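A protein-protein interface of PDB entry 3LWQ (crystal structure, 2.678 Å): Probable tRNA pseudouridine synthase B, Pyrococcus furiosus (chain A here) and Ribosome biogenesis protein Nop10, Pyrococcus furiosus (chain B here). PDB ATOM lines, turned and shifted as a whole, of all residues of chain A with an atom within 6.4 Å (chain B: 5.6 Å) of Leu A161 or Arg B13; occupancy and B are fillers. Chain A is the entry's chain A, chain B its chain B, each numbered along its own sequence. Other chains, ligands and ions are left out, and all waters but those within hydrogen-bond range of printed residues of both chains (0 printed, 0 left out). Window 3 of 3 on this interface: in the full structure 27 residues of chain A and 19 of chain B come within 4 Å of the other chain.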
ATOM      1  N   VAL A 111     -15.788  28.959 -26.738  1.00  0.00           N
ATOM      2  CA  VAL A 111     -15.079  29.564 -25.616  1.00  0.00           C
ATOM      3  C   VAL A 111     -14.885  31.009 -26.015  1.00  0.00           C
ATOM      4  O   VAL A 111     -14.372  31.295 -27.096  1.00  0.00           O
ATOM      5  CB  VAL A 111     -13.735  28.892 -25.336  1.00  0.00           C
ATOM      6  CG1 VAL A 111     -12.826  29.831 -24.637  1.00  0.00           C
ATOM      7  CG2 VAL A 111     -13.938  27.652 -24.485  1.00  0.00           C
ATOM      8  N   GLU A 159     -20.485  28.558 -18.553  1.00  0.00           N
ATOM      9  CA  GLU A 159     -19.480  28.286 -17.541  1.00  0.00           C
ATOM     10  C   GLU A 159     -18.420  29.361 -17.597  1.00  0.00           C
ATOM     11  O   GLU A 159     -17.837  29.614 -18.649  1.00  0.00           O
ATOM     12  CB  GLU A 159     -18.844  26.909 -17.765  1.00  0.00           C
ATOM     13  CG  GLU A 159     -17.801  26.510 -16.720  1.00  0.00           C
ATOM     14  CD  GLU A 159     -17.128  25.169 -17.019  1.00  0.00           C
ATOM     15  OE1 GLU A 159     -17.196  24.675 -18.177  1.00  0.00           O
ATOM     16  OE2 GLU A 159     -16.517  24.611 -16.083  1.00  0.00           O
ATOM     17  N   VAL A 160     -18.176  29.991 -16.460  1.00  0.00           N
ATOM     18  CA  VAL A 160     -17.155  31.012 -16.360  1.00  0.00           C
ATOM     19  C   VAL A 160     -15.855  30.359 -15.915  1.00  0.00           C
ATOM     20  O   VAL A 160     -15.743  29.872 -14.792  1.00  0.00           O
ATOM     21  CB  VAL A 160     -17.592  32.133 -15.400  1.00  0.00           C
ATOM     22  CG1 VAL A 160     -16.486  33.139 -15.204  1.00  0.00           C
ATOM     23  CG2 VAL A 160     -18.840  32.813 -15.937  1.00  0.00           C
ATOM     24  N   LEU A 161     -14.894  30.321 -16.826  1.00  0.00           N
ATOM     25  CA  LEU A 161     -13.616  29.674 -16.586  1.00  0.00           C
ATOM     26  C   LEU A 161     -12.823  30.505 -15.610  1.00  0.00           C
ATOM     27  O   LEU A 161     -12.442  30.051 -14.529  1.00  0.00           O
ATOM     28  CB  LEU A 161     -12.842  29.547 -17.898  1.00  0.00           C
ATOM     29  CG  LEU A 161     -13.551  28.519 -18.774  1.00  0.00           C
ATOM     30  CD1 LEU A 161     -12.789  28.192 -20.066  1.00  0.00           C
ATOM     31  CD2 LEU A 161     -13.753  27.284 -17.934  1.00  0.00           C
ATOM     32  N   GLU A 162     -12.576  31.742 -16.003  1.00  0.00           N
ATOM     33  CA  GLU A 162     -11.742  32.597 -15.200  1.00  0.00           C
ATOM     34  C   GLU A 162     -11.903  34.072 -15.538  1.00  0.00           C
ATOM     35  O   GLU A 162     -12.302  34.435 -16.646  1.00  0.00           O
ATOM     36  CB  GLU A 162     -10.288  32.144 -15.282  1.00  0.00           C
ATOM     37  CG  GLU A 162      -9.656  32.266 -16.623  1.00  0.00           C
ATOM     38  CD  GLU A 162      -8.240  31.712 -16.625  1.00  0.00           C
ATOM     39  OE1 GLU A 162      -7.324  32.491 -16.969  1.00  0.00           O
ATOM     40  OE2 GLU A 162      -8.046  30.517 -16.270  1.00  0.00           O
ATOM     41  N   ILE A 163     -11.599  34.903 -14.546  1.00  0.00           N
ATOM     42  CA  ILE A 163     -11.854  36.333 -14.573  1.00  0.00           C
ATOM     43  C   ILE A 163     -10.618  37.065 -14.097  1.00  0.00           C
ATOM     44  O   ILE A 163     -10.217  36.956 -12.924  1.00  0.00           O
ATOM     45  CB  ILE A 163     -13.036  36.704 -13.630  1.00  0.00           C
ATOM     46  CG1 ILE A 163     -14.366  36.256 -14.232  1.00  0.00           C
ATOM     47  CG2 ILE A 163     -13.079  38.201 -13.347  1.00  0.00           C
ATOM     48  CD1 ILE A 163     -15.458  36.128 -13.211  1.00  0.00           C
ATOM     49  N   VAL A 168     -13.276  38.322 -18.895  1.00  0.00           N
ATOM     50  CA  VAL A 168     -14.012  37.154 -18.476  1.00  0.00           C
ATOM     51  C   VAL A 168     -13.959  36.101 -19.548  1.00  0.00           C
ATOM     52  O   VAL A 168     -14.538  36.276 -20.610  1.00  0.00           O
ATOM     53  CB  VAL A 168     -15.465  37.497 -18.195  1.00  0.00           C
ATOM     54  CG1 VAL A 168     -16.245  36.218 -17.882  1.00  0.00           C
ATOM     55  CG2 VAL A 168     -15.531  38.485 -17.061  1.00  0.00           C
ATOM     56  N   LEU A 169     -13.250  35.011 -19.270  1.00  0.00           N
ATOM     57  CA  LEU A 169     -13.237  33.861 -20.178  1.00  0.00           C
ATOM     58  C   LEU A 169     -14.351  32.916 -19.740  1.00  0.00           C
ATOM     59  O   LEU A 169     -14.508  32.637 -18.553  1.00  0.00           O
ATOM     60  CB  LEU A 169     -11.867  33.174 -20.185  1.00  0.00           C
ATOM     61  CG  LEU A 169     -11.617  31.952 -21.070  1.00  0.00           C
ATOM     62  CD1 LEU A 169     -11.549  32.356 -22.537  1.00  0.00           C
ATOM     63  CD2 LEU A 169     -10.338  31.206 -20.650  1.00  0.00           C
ATOM     64  N   PHE A 170     -15.161  32.468 -20.687  1.00  0.00           N
ATOM     65  CA  PHE A 170     -16.252  31.565 -20.351  1.00  0.00           C
ATOM     66  C   PHE A 170     -16.553  30.639 -21.515  1.00  0.00           C
ATOM     67  O   PHE A 170     -16.243  30.955 -22.668  1.00  0.00           O
ATOM     68  CB  PHE A 170     -17.492  32.348 -19.968  1.00  0.00           C
ATOM     69  CG  PHE A 170     -18.068  33.130 -21.098  1.00  0.00           C
ATOM     70  CD1 PHE A 170     -19.260  32.743 -21.693  1.00  0.00           C
ATOM     71  CD2 PHE A 170     -17.404  34.247 -21.589  1.00  0.00           C
ATOM     72  CE1 PHE A 170     -19.792  33.469 -22.748  1.00  0.00           C
ATOM     73  CE2 PHE A 170     -17.919  34.968 -22.645  1.00  0.00           C
ATOM     74  CZ  PHE A 170     -19.119  34.580 -23.229  1.00  0.00           C
ATOM     75  N   ARG A 171     -17.108  29.472 -21.192  1.00  0.00           N
ATOM     76  CA  ARG A 171     -17.565  28.509 -22.186  1.00  0.00           C
ATOM     77  C   ARG A 171     -19.069  28.656 -22.229  1.00  0.00           C
ATOM     78  O   ARG A 171     -19.695  28.907 -21.198  1.00  0.00           O
ATOM     79  CB  ARG A 171     -17.220  27.088 -21.768  1.00  0.00           C
ATOM     80  CG  ARG A 171     -15.771  26.637 -21.968  1.00  0.00           C
ATOM     81  CD  ARG A 171     -15.651  25.116 -21.745  1.00  0.00           C
ATOM     82  NE  ARG A 171     -14.378  24.543 -22.195  1.00  0.00           N
ATOM     83  CZ  ARG A 171     -14.233  23.815 -23.303  1.00  0.00           C
ATOM     84  NH1 ARG A 171     -15.277  23.575 -24.082  1.00  0.00           N
ATOM     85  NH2 ARG A 171     -13.045  23.324 -23.640  1.00  0.00           N
ATOM     86  N   ARG B   6      -5.638  30.553 -24.111  1.00  0.00           N
ATOM     87  CA  ARG B   6      -4.643  29.491 -24.086  1.00  0.00           C
ATOM     88  C   ARG B   6      -5.284  28.159 -23.715  1.00  0.00           C
ATOM     89  O   ARG B   6      -6.466  28.098 -23.330  1.00  0.00           O
ATOM     90  CB  ARG B   6      -3.505  29.830 -23.113  1.00  0.00           C
ATOM     91  CG  ARG B   6      -2.909  31.239 -23.278  1.00  0.00           C
ATOM     92  CD  ARG B   6      -1.745  31.494 -22.302  1.00  0.00           C
ATOM     93  NE  ARG B   6      -0.552  30.705 -22.630  1.00  0.00           N
ATOM     94  CZ  ARG B   6       0.291  30.975 -23.631  1.00  0.00           C
ATOM     95  NH1 ARG B   6       0.089  32.021 -24.429  1.00  0.00           N
ATOM     96  NH2 ARG B   6       1.342  30.189 -23.843  1.00  0.00           N
ATOM     97  N   LYS B   7      -4.501  27.091 -23.825  1.00  0.00           N
ATOM     98  CA  LYS B   7      -5.027  25.751 -23.605  1.00  0.00           C
ATOM     99  C   LYS B   7      -3.969  24.770 -23.054  1.00  0.00           C
ATOM    100  O   LYS B   7      -2.852  24.700 -23.568  1.00  0.00           O
ATOM    101  CB  LYS B   7      -5.635  25.247 -24.918  1.00  0.00           C
ATOM    102  CG  LYS B   7      -6.781  24.274 -24.737  1.00  0.00           C
ATOM    103  CD  LYS B   7      -7.061  23.516 -26.019  1.00  0.00           C
ATOM    104  CE  LYS B   7      -8.133  22.458 -25.807  1.00  0.00           C
ATOM    105  NZ  LYS B   7      -8.186  21.600 -27.011  1.00  0.00           N
ATOM    106  N   CYS B   8      -4.320  24.027 -22.001  1.00  0.00           N
ATOM    107  CA  CYS B   8      -3.474  22.948 -21.441  1.00  0.00           C
ATOM    108  C   CYS B   8      -3.425  21.808 -22.483  1.00  0.00           C
ATOM    109  O   CYS B   8      -4.472  21.288 -22.898  1.00  0.00           O
ATOM    110  CB  CYS B   8      -4.083  22.493 -20.092  1.00  0.00           C
ATOM    111  SG  CYS B   8      -3.305  21.221 -18.953  1.00  0.00           S
ATOM    112  N   CYS B  11      -4.708  18.348 -20.043  1.00  0.00           N
ATOM    113  CA  CYS B  11      -6.115  18.453 -19.604  1.00  0.00           C
ATOM    114  C   CYS B  11      -7.117  18.907 -20.672  1.00  0.00           C
ATOM    115  O   CYS B  11      -8.292  18.547 -20.591  1.00  0.00           O
ATOM    116  CB  CYS B  11      -6.285  19.355 -18.346  1.00  0.00           C
ATOM    117  SG  CYS B  11      -5.002  20.585 -18.003  1.00  0.00           S
ATOM    118  N   GLY B  12      -6.674  19.725 -21.630  1.00  0.00           N
ATOM    119  CA  GLY B  12      -7.571  20.375 -22.590  1.00  0.00           C
ATOM    120  C   GLY B  12      -8.347  21.572 -22.030  1.00  0.00           C
ATOM    121  O   GLY B  12      -9.336  22.035 -22.603  1.00  0.00           O
ATOM    122  N   ARG B  13      -7.899  22.065 -20.885  1.00  0.00           N
ATOM    123  CA  ARG B  13      -8.515  23.201 -20.218  1.00  0.00           C
ATOM    124  C   ARG B  13      -8.179  24.545 -20.906  1.00  0.00           C
ATOM    125  O   ARG B  13      -7.065  24.748 -21.416  1.00  0.00           O
ATOM    126  CB  ARG B  13      -8.058  23.201 -18.759  1.00  0.00           C
ATOM    127  CG  ARG B  13      -8.293  24.459 -18.008  1.00  0.00           C
ATOM    128  CD  ARG B  13      -9.757  24.720 -17.720  1.00  0.00           C
ATOM    129  NE  ARG B  13      -9.867  26.029 -17.081  1.00  0.00           N
ATOM    130  CZ  ARG B  13     -10.168  26.225 -15.803  1.00  0.00           C
ATOM    131  NH1 ARG B  13     -10.442  25.187 -15.013  1.00  0.00           N
ATOM    132  NH2 ARG B  13     -10.210  27.469 -15.326  1.00  0.00           N
ATOM    133  N   TYR B  14      -9.153  25.451 -20.924  1.00  0.00           N
ATOM    134  CA  TYR B  14      -8.957  26.788 -21.487  1.00  0.00           C
ATOM    135  C   TYR B  14      -8.660  27.816 -20.402  1.00  0.00           C
ATOM    136  O   TYR B  14      -9.261  27.807 -19.332  1.00  0.00           O
ATOM    137  CB  TYR B  14     -10.174  27.218 -22.295  1.00  0.00           C
ATOM    138  CG  TYR B  14     -10.153  26.710 -23.703  1.00  0.00           C
ATOM    139  CD1 TYR B  14     -10.905  25.600 -24.081  1.00  0.00           C
ATOM    140  CD2 TYR B  14      -9.369  27.333 -24.661  1.00  0.00           C
ATOM    141  CE1 TYR B  14     -10.881  25.139 -25.389  1.00  0.00           C
ATOM    142  CE2 TYR B  14      -9.333  26.883 -25.960  1.00  0.00           C
ATOM    143  CZ  TYR B  14     -10.086  25.793 -26.324  1.00  0.00           C
ATOM    144  OH  TYR B  14     -10.031  25.364 -27.635  1.00  0.00           O
ATOM    145  N   THR B  15      -7.736  28.712 -20.691  1.00  0.00           N
ATOM    146  CA  THR B  15      -7.248  29.586 -19.662  1.00  0.00           C
ATOM    147  C   THR B  15      -6.516  30.789 -20.281  1.00  0.00           C
ATOM    148  O   THR B  15      -6.153  30.767 -21.461  1.00  0.00           O
ATOM    149  CB  THR B  15      -6.351  28.770 -18.692  1.00  0.00           C
ATOM    150  OG1 THR B  15      -5.633  29.639 -17.801  1.00  0.00           O
ATOM    151  CG2 THR B  15      -5.373  27.941 -19.480  1.00  0.00           C
ATOM    152  N   CYS B  20      -1.371  25.509 -16.665  1.00  0.00           N
ATOM    153  CA  CYS B  20      -2.634  24.784 -16.460  1.00  0.00           C
ATOM    154  C   CYS B  20      -2.924  24.870 -14.966  1.00  0.00           C
ATOM    155  O   CYS B  20      -2.125  24.417 -14.141  1.00  0.00           O
ATOM    156  CB  CYS B  20      -2.484  23.314 -16.926  1.00  0.00           C
ATOM    157  SG  CYS B  20      -3.962  22.163 -17.214  1.00  0.00           S
ATOM    158  N   PRO B  21      -4.046  25.501 -14.603  1.00  0.00           N
ATOM    159  CA  PRO B  21      -4.416  25.548 -13.185  1.00  0.00           C
ATOM    160  C   PRO B  21      -5.129  24.246 -12.792  1.00  0.00           C
ATOM    161  O   PRO B  21      -5.524  24.076 -11.642  1.00  0.00           O
ATOM    162  CB  PRO B  21      -5.387  26.739 -13.101  1.00  0.00           C
ATOM    163  CG  PRO B  21      -5.713  27.107 -14.557  1.00  0.00           C
ATOM    164  CD  PRO B  21      -5.065  26.112 -15.468  1.00  0.00           C
ATOM    165  N   VAL B  22      -5.292  23.352 -13.763  1.00  0.00           N
ATOM    166  CA  VAL B  22      -5.853  22.022 -13.542  1.00  0.00           C
ATOM    167  C   VAL B  22      -4.737  20.996 -13.286  1.00  0.00           C
ATOM    168  O   VAL B  22      -4.723  20.322 -12.264  1.00  0.00           O
ATOM    169  CB  VAL B  22      -6.710  21.565 -14.771  1.00  0.00           C
ATOM    170  CG1 VAL B  22      -6.826  20.048 -14.829  1.00  0.00           C
ATOM    171  CG2 VAL B  22      -8.094  22.222 -14.757  1.00  0.00           C
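N of Leu A161 lies within hydrogen-bond range of O of Leu A169.
O of Glu A162 lies within hydrogen-bond range of N of Leu A169, 2.8 Å away.
O of Arg B13 lies within hydrogen-bond range of N of Cys B8 (2.9 Å).
SG of Cys B8 is disulfide-bonded to SG of Cys B11.
SG of Cys B8 is disulfide-bonded to SG of Cys B20, at 2.1 Å.
The side-chain sulfur (SG) of Cys B11 forms a disulfide with the side-chain sulfur (SG) of Cys B20, at 2.0 Å.
The guanidinium group (NH2) of Arg B13 is in salt-bridge range of the side-chain carboxylate (OE2) of Glu A162.
The side-chain carboxylate of Glu A162 lies within hydrogen-bond range of the side-chain hydroxyl of Thr B15, at 3.0 Å.
Leu A161 touches two residues of chain B.
Arg B13 touches just these residues of chain A: Leu A161 (3.5 Å) and Glu A162 (3.9 Å).
Printed residues of chain B within 4 Å of Glu A162: Arg B13 (3.9 Å) and Thr B15 (3.0 Å).
Of the printed residues of chain B, Val A111 touches Tyr B14 (3.7 Å).
Of the printed residues of chain A, Thr B15 touches Glu A162 (3.0 Å) and Leu A169 (3.6 Å).
Of the printed residues of chain B, Leu A169 touches Tyr B14 and Thr B15.
Of the printed residues of chain A, Tyr B14 touches Val A111, Leu A161, Leu A169 and Arg A171.
Cys B20 touches none of the printed residues of chain A.
Cys B11 touches none of the printed residues of chain A.
The nearest residue of chain A that does not touch Arg B13 is Arg A171 (5.7 Å).
The nearest printed residue of chain B that does not touch Glu A162 is Tyr B14 (4.3 Å).
CD1 of Tyr B14 touches CG2 of Val A111, 3.7 Å away.
Leu A161 touches Arg B13.
Tyr B14 touches Leu A161.
C of Tyr B14 touches CD2 of Leu A169 (3.8 Å).
Leu A169 touches Thr B15.
Tyr B14 touches Arg A171.
Among the printed residues, Asp or Glu carboxylates within 4 Å of a Lys or Arg side-chain nitrogen of the other chain: Glu A162 with Arg B13.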
